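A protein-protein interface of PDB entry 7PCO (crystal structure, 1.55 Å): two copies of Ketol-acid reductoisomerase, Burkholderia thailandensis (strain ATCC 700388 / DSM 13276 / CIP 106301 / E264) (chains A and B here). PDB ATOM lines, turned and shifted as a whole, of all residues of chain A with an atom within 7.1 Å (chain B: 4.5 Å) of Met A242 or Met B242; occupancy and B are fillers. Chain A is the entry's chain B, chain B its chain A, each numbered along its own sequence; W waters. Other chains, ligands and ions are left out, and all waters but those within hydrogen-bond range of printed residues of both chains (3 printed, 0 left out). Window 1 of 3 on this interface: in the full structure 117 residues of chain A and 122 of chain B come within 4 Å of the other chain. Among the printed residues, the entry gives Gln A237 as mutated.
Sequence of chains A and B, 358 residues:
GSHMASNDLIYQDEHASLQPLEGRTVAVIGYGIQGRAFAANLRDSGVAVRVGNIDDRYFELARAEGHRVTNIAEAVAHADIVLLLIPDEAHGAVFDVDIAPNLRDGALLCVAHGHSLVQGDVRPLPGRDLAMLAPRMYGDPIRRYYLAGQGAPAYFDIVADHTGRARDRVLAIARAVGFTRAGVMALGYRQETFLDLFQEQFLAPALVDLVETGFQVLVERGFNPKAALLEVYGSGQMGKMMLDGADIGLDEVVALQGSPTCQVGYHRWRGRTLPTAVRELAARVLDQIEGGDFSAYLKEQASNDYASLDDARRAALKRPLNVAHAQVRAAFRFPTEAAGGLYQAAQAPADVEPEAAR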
ATOM      1  N   TYR A 138      22.950 -27.335   6.224  1.00  0.00           N
ATOM      2  CA  TYR A 138      21.902 -28.367   6.064  1.00  0.00           C
ATOM      3  C   TYR A 138      22.569 -29.752   6.078  1.00  0.00           C
ATOM      4  O   TYR A 138      23.801 -29.852   6.189  1.00  0.00           O
ATOM      5  CB  TYR A 138      20.989 -28.046   4.874  1.00  0.00           C
ATOM      6  CG  TYR A 138      21.604 -27.686   3.545  1.00  0.00           C
ATOM      7  CD1 TYR A 138      21.827 -28.649   2.573  1.00  0.00           C
ATOM      8  CD2 TYR A 138      21.807 -26.362   3.196  1.00  0.00           C
ATOM      9  CE1 TYR A 138      22.320 -28.317   1.316  1.00  0.00           C
ATOM     10  CE2 TYR A 138      22.303 -26.014   1.950  1.00  0.00           C
ATOM     11  CZ  TYR A 138      22.555 -26.991   1.002  1.00  0.00           C
ATOM     12  OH  TYR A 138      23.023 -26.613  -0.229  1.00  0.00           O
ATOM     13  N   LEU A 207      19.381 -12.939  -2.689  1.00  0.00           N
ATOM     14  CA  LEU A 207      20.401 -13.542  -3.590  1.00  0.00           C
ATOM     15  C   LEU A 207      19.670 -14.157  -4.792  1.00  0.00           C
ATOM     16  O   LEU A 207      20.088 -13.938  -5.942  1.00  0.00           O
ATOM     17  CB  LEU A 207      21.225 -14.612  -2.863  1.00  0.00           C
ATOM     18  CG  LEU A 207      22.237 -14.129  -1.819  1.00  0.00           C
ATOM     19  CD1 LEU A 207      22.833 -15.325  -1.096  1.00  0.00           C
ATOM     20  CD2 LEU A 207      23.353 -13.273  -2.420  1.00  0.00           C
ATOM     21  N   VAL A 208      18.615 -14.928  -4.539  1.00  0.00           N
ATOM     22  CA  VAL A 208      17.876 -15.608  -5.643  1.00  0.00           C
ATOM     23  C   VAL A 208      17.180 -14.541  -6.495  1.00  0.00           C
ATOM     24  O   VAL A 208      17.204 -14.673  -7.731  1.00  0.00           O
ATOM     25  CB  VAL A 208      16.929 -16.701  -5.119  1.00  0.00           C
ATOM     26  CG1 VAL A 208      16.170 -17.377  -6.253  1.00  0.00           C
ATOM     27  CG2 VAL A 208      17.696 -17.745  -4.328  1.00  0.00           C
ATOM     28  N   VAL A 211      19.845 -13.069  -8.821  1.00  0.00           N
ATOM     29  CA  VAL A 211      20.121 -14.067  -9.894  1.00  0.00           C
ATOM     30  C   VAL A 211      18.987 -13.965 -10.922  1.00  0.00           C
ATOM     31  O   VAL A 211      19.268 -13.910 -12.137  1.00  0.00           O
ATOM     32  CB  VAL A 211      20.246 -15.480  -9.289  1.00  0.00           C
ATOM     33  CG1 VAL A 211      20.130 -16.589 -10.321  1.00  0.00           C
ATOM     34  CG2 VAL A 211      21.530 -15.634  -8.499  1.00  0.00           C
ATOM     35  N   VAL A 232      23.974 -16.825 -14.764  1.00  0.00           N
ATOM     36  CA  VAL A 232      23.490 -16.248 -13.477  1.00  0.00           C
ATOM     37  C   VAL A 232      23.620 -17.293 -12.353  1.00  0.00           C
ATOM     38  O   VAL A 232      23.810 -16.873 -11.214  1.00  0.00           O
ATOM     39  CB  VAL A 232      22.092 -15.605 -13.586  1.00  0.00           C
ATOM     40  CG1 VAL A 232      22.103 -14.472 -14.611  1.00  0.00           C
ATOM     41  CG2 VAL A 232      20.990 -16.609 -13.879  1.00  0.00           C
ATOM     42  N   TYR A 233      23.632 -18.598 -12.640  1.00  0.00           N
ATOM     43  CA  TYR A 233      24.000 -19.619 -11.618  1.00  0.00           C
ATOM     44  C   TYR A 233      24.176 -21.020 -12.214  1.00  0.00           C
ATOM     45  O   TYR A 233      24.888 -21.817 -11.589  1.00  0.00           O
ATOM     46  CB  TYR A 233      22.957 -19.683 -10.491  1.00  0.00           C
ATOM     47  CG  TYR A 233      21.687 -20.389 -10.897  1.00  0.00           C
ATOM     48  CD1 TYR A 233      20.664 -19.725 -11.552  1.00  0.00           C
ATOM     49  CD2 TYR A 233      21.520 -21.740 -10.650  1.00  0.00           C
ATOM     50  CE1 TYR A 233      19.520 -20.384 -11.974  1.00  0.00           C
ATOM     51  CE2 TYR A 233      20.381 -22.416 -11.066  1.00  0.00           C
ATOM     52  CZ  TYR A 233      19.369 -21.734 -11.721  1.00  0.00           C
ATOM     53  OH  TYR A 233      18.236 -22.374 -12.144  1.00  0.00           O
ATOM     54  N   GLY A 234      23.520 -21.342 -13.342  1.00  0.00           N
ATOM     55  CA  GLY A 234      23.369 -22.724 -13.824  1.00  0.00           C
ATOM     56  C   GLY A 234      24.687 -23.406 -14.143  1.00  0.00           C
ATOM     57  O   GLY A 234      24.728 -24.650 -14.103  1.00  0.00           O
ATOM     58  N   GLY A 236      27.246 -23.250 -12.329  1.00  0.00           N
ATOM     59  CA  GLY A 236      27.871 -23.457 -11.006  1.00  0.00           C
ATOM     60  C   GLY A 236      28.931 -22.419 -10.696  1.00  0.00           C
ATOM     61  O   GLY A 236      29.480 -22.471  -9.574  1.00  0.00           O
ATOM     62  N   GLN A 237      29.238 -21.499 -11.622  1.00  0.00           N
ATOM     63  CA  GLN A 237      30.343 -20.541 -11.372  1.00  0.00           C
ATOM     64  C   GLN A 237      29.998 -19.620 -10.198  1.00  0.00           C
ATOM     65  O   GLN A 237      30.899 -19.382  -9.366  1.00  0.00           O
ATOM     66  CB  GLN A 237      30.696 -19.675 -12.570  1.00  0.00           C
ATOM     67  CG  GLN A 237      31.911 -18.808 -12.274  1.00  0.00           C
ATOM     68  CD  GLN A 237      32.528 -18.264 -13.533  1.00  0.00           C
ATOM     69  OE1 GLN A 237      31.961 -17.401 -14.194  1.00  0.00           O
ATOM     70  NE2 GLN A 237      33.706 -18.766 -13.867  1.00  0.00           N
ATOM     71  N   MET A 238      28.803 -19.031 -10.164  1.00  0.00           N
ATOM     72  CA  MET A 238      28.465 -18.096  -9.062  1.00  0.00           C
ATOM     73  C   MET A 238      28.447 -18.862  -7.731  1.00  0.00           C
ATOM     74  O   MET A 238      28.980 -18.313  -6.734  1.00  0.00           O
ATOM     75  CB  MET A 238      27.144 -17.361  -9.307  1.00  0.00           C
ATOM     76  CG  MET A 238      27.201 -16.408 -10.494  1.00  0.00           C
ATOM     77  SD  MET A 238      28.314 -14.983 -10.296  1.00  0.00           S
ATOM     78  CE  MET A 238      29.842 -15.645 -10.959  1.00  0.00           C
ATOM     79  N   GLY A 239      27.920 -20.094  -7.709  1.00  0.00           N
ATOM     80  CA  GLY A 239      27.953 -20.952  -6.511  1.00  0.00           C
ATOM     81  C   GLY A 239      29.382 -21.237  -6.071  1.00  0.00           C
ATOM     82  O   GLY A 239      29.695 -21.075  -4.862  1.00  0.00           O
ATOM     83  N   LYS A 240      30.231 -21.656  -7.011  1.00  0.00           N
ATOM     84  CA  LYS A 240      31.660 -21.965  -6.744  1.00  0.00           C
ATOM     85  C   LYS A 240      32.354 -20.715  -6.171  1.00  0.00           C
ATOM     86  O   LYS A 240      33.124 -20.858  -5.214  1.00  0.00           O
ATOM     87  CB  LYS A 240      32.363 -22.464  -8.007  1.00  0.00           C
ATOM     88  CG  LYS A 240      32.541 -23.970  -8.119  1.00  0.00           C
ATOM     89  CD  LYS A 240      33.171 -24.607  -6.901  1.00  0.00           C
ATOM     90  CE  LYS A 240      34.195 -25.659  -7.255  1.00  0.00           C
ATOM     91  NZ  LYS A 240      34.227 -26.749  -6.254  1.00  0.00           N
ATOM     92  N   MET A 241      32.075 -19.530  -6.727  1.00  0.00           N
ATOM     93  CA  MET A 241      32.645 -18.233  -6.270  1.00  0.00           C
ATOM     94  C   MET A 241      32.289 -18.007  -4.794  1.00  0.00           C
ATOM     95  O   MET A 241      33.183 -17.627  -3.992  1.00  0.00           O
ATOM     96  CB  MET A 241      32.106 -17.069  -7.112  1.00  0.00           C
ATOM     97  CG  MET A 241      32.710 -15.735  -6.752  1.00  0.00           C
ATOM     98  SD  MET A 241      31.896 -14.305  -7.518  1.00  0.00           S
ATOM     99  CE  MET A 241      30.348 -14.290  -6.614  1.00  0.00           C
ATOM    100  N   MET A 242      31.026 -18.230  -4.441  1.00  0.00           N
ATOM    101  CA  MET A 242      30.504 -17.985  -3.074  1.00  0.00           C
ATOM    102  C   MET A 242      31.021 -19.049  -2.103  1.00  0.00           C
ATOM    103  O   MET A 242      31.241 -18.702  -0.921  1.00  0.00           O
ATOM    104  CB  MET A 242      28.979 -17.993  -3.086  1.00  0.00           C
ATOM    105  CG  MET A 242      28.430 -16.981  -4.031  1.00  0.00           C
ATOM    106  SD  MET A 242      26.875 -16.323  -3.472  1.00  0.00           S
ATOM    107  CE  MET A 242      27.565 -15.107  -2.355  1.00  0.00           C
ATOM    108  N   LEU A 243      31.210 -20.285  -2.562  1.00  0.00           N
ATOM    109  CA  LEU A 243      31.684 -21.380  -1.684  1.00  0.00           C
ATOM    110  C   LEU A 243      33.203 -21.286  -1.503  1.00  0.00           C
ATOM    111  O   LEU A 243      33.666 -21.399  -0.357  1.00  0.00           O
ATOM    112  CB  LEU A 243      31.244 -22.724  -2.263  1.00  0.00           C
ATOM    113  CG  LEU A 243      31.464 -23.934  -1.362  1.00  0.00           C
ATOM    114  CD1 LEU A 243      30.685 -23.804  -0.057  1.00  0.00           C
ATOM    115  CD2 LEU A 243      31.073 -25.209  -2.096  1.00  0.00           C
ATOM    116  N   ASP A 244      33.960 -21.026  -2.572  1.00  0.00           N
ATOM    117  CA  ASP A 244      35.415 -20.744  -2.445  1.00  0.00           C
ATOM    118  C   ASP A 244      35.597 -19.463  -1.621  1.00  0.00           C
ATOM    119  O   ASP A 244      36.573 -19.384  -0.856  1.00  0.00           O
ATOM    120  CB  ASP A 244      36.088 -20.647  -3.815  1.00  0.00           C
ATOM    121  CG  ASP A 244      36.240 -21.964  -4.562  1.00  0.00           C
ATOM    122  OD1 ASP A 244      35.947 -23.034  -3.978  1.00  0.00           O
ATOM    123  OD2 ASP A 244      36.659 -21.904  -5.723  1.00  0.00           O
ATOM    124  N   GLY A 245      34.702 -18.488  -1.788  1.00  0.00           N
ATOM    125  CA  GLY A 245      34.753 -17.201  -1.069  1.00  0.00           C
ATOM    126  C   GLY A 245      34.628 -17.421   0.424  1.00  0.00           C
ATOM    127  O   GLY A 245      35.287 -16.707   1.179  1.00  0.00           O
ATOM    128  N   ALA A 246      33.828 -18.404   0.841  1.00  0.00           N
ATOM    129  CA  ALA A 246      33.699 -18.779   2.266  1.00  0.00           C
ATOM    130  C   ALA A 246      35.081 -19.156   2.811  1.00  0.00           C
ATOM    131  O   ALA A 246      35.380 -18.815   3.958  1.00  0.00           O
ATOM    132  CB  ALA A 246      32.705 -19.904   2.425  1.00  0.00           C
ATOM    133  N   ASP A 247      35.900 -19.838   2.014  1.00  0.00           N
ATOM    134  CA  ASP A 247      37.269 -20.243   2.417  1.00  0.00           C
ATOM    135  C   ASP A 247      38.168 -19.003   2.499  1.00  0.00           C
ATOM    136  O   ASP A 247      38.674 -18.697   3.608  1.00  0.00           O
ATOM    137  CB  ASP A 247      37.832 -21.281   1.449  1.00  0.00           C
ATOM    138  CG  ASP A 247      39.115 -21.938   1.911  1.00  0.00           C
ATOM    139  OD1 ASP A 247      39.485 -21.764   3.098  1.00  0.00           O
ATOM    140  OD2 ASP A 247      39.732 -22.615   1.074  1.00  0.00           O
ATOM    141  N   LEU A 250      35.538 -13.256  -0.538  1.00  0.00           N
ATOM    142  CA  LEU A 250      34.828 -13.094  -1.833  1.00  0.00           C
ATOM    143  C   LEU A 250      35.664 -12.215  -2.768  1.00  0.00           C
ATOM    144  O   LEU A 250      35.812 -12.565  -3.959  1.00  0.00           O
ATOM    145  CB  LEU A 250      33.435 -12.526  -1.577  1.00  0.00           C
ATOM    146  CG  LEU A 250      32.490 -13.516  -0.896  1.00  0.00           C
ATOM    147  CD1 LEU A 250      31.332 -12.773  -0.260  1.00  0.00           C
ATOM    148  CD2 LEU A 250      31.993 -14.580  -1.877  1.00  0.00           C
ATOM    149  N   VAL A 253      38.655 -14.332  -4.027  1.00  0.00           N
ATOM    150  CA  VAL A 253      38.371 -15.307  -5.126  1.00  0.00           C
ATOM    151  C   VAL A 253      38.510 -14.591  -6.467  1.00  0.00           C
ATOM    152  O   VAL A 253      39.097 -15.146  -7.400  1.00  0.00           O
ATOM    153  CB  VAL A 253      36.982 -15.954  -5.025  1.00  0.00           C
ATOM    154  CG1 VAL A 253      36.675 -16.759  -6.275  1.00  0.00           C
ATOM    155  CG2 VAL A 253      36.865 -16.813  -3.796  1.00  0.00           C
ATOM    156  N   PHE A 334      25.572 -31.812 -15.201  1.00  0.00           N
ATOM    157  CA  PHE A 334      26.151 -31.104 -14.031  1.00  0.00           C
ATOM    158  C   PHE A 334      26.959 -32.110 -13.221  1.00  0.00           C
ATOM    159  O   PHE A 334      26.513 -33.230 -13.018  1.00  0.00           O
ATOM    160  CB  PHE A 334      25.066 -30.465 -13.159  1.00  0.00           C
ATOM    161  CG  PHE A 334      25.633 -29.521 -12.130  1.00  0.00           C
ATOM    162  CD1 PHE A 334      26.106 -28.274 -12.508  1.00  0.00           C
ATOM    163  CD2 PHE A 334      25.755 -29.902 -10.803  1.00  0.00           C
ATOM    164  CE1 PHE A 334      26.668 -27.418 -11.575  1.00  0.00           C
ATOM    165  CE2 PHE A 334      26.307 -29.041  -9.870  1.00  0.00           C
ATOM    166  CZ  PHE A 334      26.767 -27.805 -10.258  1.00  0.00           C
ATOM    167  N   LEU B 207      25.988  -9.618  -6.015  1.00  0.00           N
ATOM    168  CA  LEU B 207      25.885 -10.742  -5.046  1.00  0.00           C
ATOM    169  C   LEU B 207      26.792 -10.423  -3.845  1.00  0.00           C
ATOM    170  O   LEU B 207      26.337 -10.553  -2.686  1.00  0.00           O
ATOM    171  CB  LEU B 207      26.281 -12.073  -5.696  1.00  0.00           C
ATOM    172  CG  LEU B 207      25.293 -12.678  -6.699  1.00  0.00           C
ATOM    173  CD1 LEU B 207      25.899 -13.906  -7.355  1.00  0.00           C
ATOM    174  CD2 LEU B 207      23.967 -13.052  -6.047  1.00  0.00           C
ATOM    175  N   VAL B 211      25.623  -9.591   0.130  1.00  0.00           N
ATOM    176  CA  VAL B 211      26.239 -10.323   1.267  1.00  0.00           C
ATOM    177  C   VAL B 211      26.813  -9.281   2.241  1.00  0.00           C
ATOM    178  O   VAL B 211      26.597  -9.401   3.462  1.00  0.00           O
ATOM    179  CB  VAL B 211      27.311 -11.297   0.736  1.00  0.00           C
ATOM    180  CG1 VAL B 211      28.355 -11.635   1.777  1.00  0.00           C
ATOM    181  CG2 VAL B 211      26.695 -12.559   0.146  1.00  0.00           C
ATOM    182  N   MET B 238      25.413 -20.289   2.079  1.00  0.00           N
ATOM    183  CA  MET B 238      24.856 -19.531   0.925  1.00  0.00           C
ATOM    184  C   MET B 238      25.508 -20.016  -0.382  1.00  0.00           C
ATOM    185  O   MET B 238      24.765 -20.222  -1.375  1.00  0.00           O
ATOM    186  CB  MET B 238      25.014 -18.022   1.134  1.00  0.00           C
ATOM    187  CG  MET B 238      24.140 -17.501   2.273  1.00  0.00           C
ATOM    188  SD  MET B 238      22.367 -17.649   1.926  1.00  0.00           S
ATOM    189  CE  MET B 238      21.971 -19.212   2.704  1.00  0.00           C
ATOM    190  N   GLY B 239      26.807 -20.331  -0.370  1.00  0.00           N
ATOM    191  CA  GLY B 239      27.501 -20.880  -1.547  1.00  0.00           C
ATOM    192  C   GLY B 239      27.013 -22.284  -1.868  1.00  0.00           C
ATOM    193  O   GLY B 239      26.781 -22.574  -3.055  1.00  0.00           O
ATOM    194  N   LYS B 240      26.825 -23.131  -0.856  1.00  0.00           N
ATOM    195  CA  LYS B 240      26.320 -24.517  -1.062  1.00  0.00           C
ATOM    196  C   LYS B 240      24.916 -24.463  -1.678  1.00  0.00           C
ATOM    197  O   LYS B 240      24.639 -25.247  -2.616  1.00  0.00           O
ATOM    198  CB  LYS B 240      26.351 -25.290   0.257  1.00  0.00           C
ATOM    199  CG  LYS B 240      26.238 -26.807   0.159  1.00  0.00           C
ATOM    200  CD  LYS B 240      27.233 -27.476  -0.771  1.00  0.00           C
ATOM    201  CE  LYS B 240      28.432 -28.096  -0.088  1.00  0.00           C
ATOM    202  NZ  LYS B 240      28.966 -29.210  -0.907  1.00  0.00           N
ATOM    203  N   MET B 241      24.064 -23.551  -1.202  1.00  0.00           N
ATOM    204  CA  MET B 241      22.702 -23.351  -1.768  1.00  0.00           C
ATOM    205  C   MET B 241      22.827 -22.979  -3.253  1.00  0.00           C
ATOM    206  O   MET B 241      22.107 -23.559  -4.087  1.00  0.00           O
ATOM    207  CB  MET B 241      21.956 -22.255  -1.005  1.00  0.00           C
ATOM    208  CG  MET B 241      20.573 -21.950  -1.553  1.00  0.00           C
ATOM    209  SD  MET B 241      19.846 -20.483  -0.780  1.00  0.00           S
ATOM    210  CE  MET B 241      20.743 -19.212  -1.674  1.00  0.00           C
ATOM    211  N   MET B 242      23.743 -22.074  -3.586  1.00  0.00           N
ATOM    212  CA  MET B 242      23.897 -21.563  -4.970  1.00  0.00           C
ATOM    213  C   MET B 242      24.510 -22.633  -5.884  1.00  0.00           C
ATOM    214  O   MET B 242      24.067 -22.745  -7.046  1.00  0.00           O
ATOM    215  CB  MET B 242      24.737 -20.293  -4.954  1.00  0.00           C
ATOM    216  CG  MET B 242      23.966 -19.168  -4.343  1.00  0.00           C
ATOM    217  SD  MET B 242      24.657 -17.601  -4.788  1.00  0.00           S
ATOM    218  CE  MET B 242      24.058 -17.549  -6.479  1.00  0.00           C
ATOM    219  N   LEU B 243      25.409 -23.460  -5.359  1.00  0.00           N
ATOM    220  CA  LEU B 243      26.078 -24.523  -6.146  1.00  0.00           C
ATOM    221  C   LEU B 243      25.147 -25.731  -6.300  1.00  0.00           C
ATOM    222  O   LEU B 243      24.990 -26.225  -7.427  1.00  0.00           O
ATOM    223  CB  LEU B 243      27.380 -24.900  -5.448  1.00  0.00           C
ATOM    224  CG  LEU B 243      28.260 -25.889  -6.198  1.00  0.00           C
ATOM    225  CD1 LEU B 243      28.544 -25.426  -7.628  1.00  0.00           C
ATOM    226  CD2 LEU B 243      29.550 -26.127  -5.437  1.00  0.00           C
ATOM    227  N   ASP B 244      24.500 -26.172  -5.223  1.00  0.00           N
ATOM    228  CA  ASP B 244      23.449 -27.218  -5.313  1.00  0.00           C
ATOM    229  C   ASP B 244      22.310 -26.696  -6.194  1.00  0.00           C
ATOM    230  O   ASP B 244      21.690 -27.508  -6.895  1.00  0.00           O
ATOM    231  CB  ASP B 244      22.912 -27.613  -3.934  1.00  0.00           C
ATOM    232  CG  ASP B 244      23.843 -28.475  -3.108  1.00  0.00           C
ATOM    233  OD1 ASP B 244      24.879 -28.912  -3.648  1.00  0.00           O
ATOM    234  OD2 ASP B 244      23.527 -28.677  -1.917  1.00  0.00           O
ATOM    235  N   GLY B 245      21.997 -25.399  -6.129  1.00  0.00           N
ATOM    236  CA  GLY B 245      20.932 -24.807  -6.963  1.00  0.00           C
ATOM    237  C   GLY B 245      21.256 -24.961  -8.439  1.00  0.00           C
ATOM    238  O   GLY B 245      20.339 -25.191  -9.231  1.00  0.00           O
ATOM    239  N   ALA B 246      22.532 -24.862  -8.813  1.00  0.00           N
ATOM    240  CA  ALA B 246      22.968 -25.126 -10.199  1.00  0.00           C
ATOM    241  C   ALA B 246      22.443 -26.497 -10.628  1.00  0.00           C
ATOM    242  O   ALA B 246      21.989 -26.613 -11.770  1.00  0.00           O
ATOM    243  CB  ALA B 246      24.465 -25.030 -10.337  1.00  0.00           C
ATOM    244  N   LEU B 250      17.180 -23.214  -7.631  1.00  0.00           N
ATOM    245  CA  LEU B 250      17.426 -22.467  -6.366  1.00  0.00           C
ATOM    246  C   LEU B 250      16.195 -22.602  -5.457  1.00  0.00           C
ATOM    247  O   LEU B 250      16.373 -22.893  -4.267  1.00  0.00           O
ATOM    248  CB  LEU B 250      17.765 -21.008  -6.680  1.00  0.00           C
ATOM    249  CG  LEU B 250      19.123 -20.817  -7.349  1.00  0.00           C
ATOM    250  CD1 LEU B 250      19.195 -19.484  -8.087  1.00  0.00           C
ATOM    251  CD2 LEU B 250      20.252 -20.943  -6.328  1.00  0.00           C
HETATM  252  O   HOH W   1      25.825 -21.554  -9.027  1.00  0.00           O
HETATM  253  O   HOH W   2      29.178 -19.250   0.993  1.00  0.00           O
HETATM  254  O   HOH W   3      16.447 -21.807 -10.068  1.00  0.00           O
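Water W1 lies within hydrogen-bond range of the backbone carbonyl oxygen of Tyr A233, the backbone NH of Gly A239 and the backbone carbonyl oxygen of Met B242. Water W3 bridges OH of Tyr A233 (2.8 Å) and N of Leu B250 (2.9 Å). Water W2 lies within hydrogen-bond range of the backbone carbonyl oxygen (O) of Met A242 and the backbone NH (N) of Gly B239.
Met A242 touches just these residues of chain B: Val B211, Gly B239 and Met B242. Of chain A, only Val A211 (3.8 Å), Gly A239 (3.6 Å) and Met A242 (2.9 Å) come within 4 Å of Met B242. Of the printed residues of chain A, Leu B243 touches Gly A236, Gly A239, Leu A243 and Phe A334. Of the printed residues of chain B, Leu A250 touches Val B211 (3.8 Å). Of the printed residues of chain A, Val B211 touches Met A242 and Leu A250. Of the printed residues of chain B, Leu A207 touches Leu B207 and Met B238. Met A241 touches none of the printed residues of chain B. The nearest residue of chain A that does not touch Met B242 is Met A238 (4.2 Å).
Printed residues of chain B that touch a printed residue of chain A: Leu B207, Val B211, Met B238, Gly B239, Lys B240, Met B241, Met B242, Leu B243, Asp B244, Gly B245, Ala B246 and Leu B250. Hydrophobic or aromatic side chains of chain B that line the printed part of chain A: Leu B207, Val B211, Met B238, Met B242, Leu B243, Ala B246 and Leu B250.
OH of Tyr A138 sits at hydrogen-bond distance from O of Lys B240. The side-chain sulfur (SD) of Met A242 lies close to the side-chain sulfur (SD) of Met B242, 2.9 Å away. The side-chain hydroxyl (OH) of Tyr A138 is in hydrogen-bond range of the backbone NH (N) of Met B241, 3.4 Å away. The side-chain carboxylate of Asp B244 sits at hydrogen-bond distance from the side-chain hydroxyl of Tyr A138, at 2.7 Å.
Val A208 touches Leu B250 (CG1 to CB, 3.99 Å). Met B242 touches Val A211 (CE to CG2, 3.8 Å). O of Gly B245 touches CE2 of Tyr A233 (3.3 Å). Ala B246 touches Gly A234 (CB to O, 3.8 Å). Leu B243 touches Gly A236. Ala B246 touches Gly A236 (CB to CA, 3.8 Å). SD of Met A238 touches CD1 of Leu B207, 3.95 Å away. Gly A239 touches Gly B239 (O to O, 3.7 Å). Lys B240 touches Leu A243 (N to CD1, 3.999 Å). Val B211 touches Leu A250 (CG1 to CD1, 3.8 Å).
Leu B207 touches its own counterpart, Leu A207. Val A211 touches Leu B250, and with the chains exchanged Leu A250 touches Val B211. Gly A239 touches its own counterpart, Gly B239. Leu A243 touches its own counterpart, Leu B243. Positions printed for both chains: 207, 211, 238, 239, 240, 241, 242, 243, 244, 245, 246 and 250. Of the 27 pairs that touch across the chains among the printed residues, 14 have their exchanged pair printed and touching as well.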
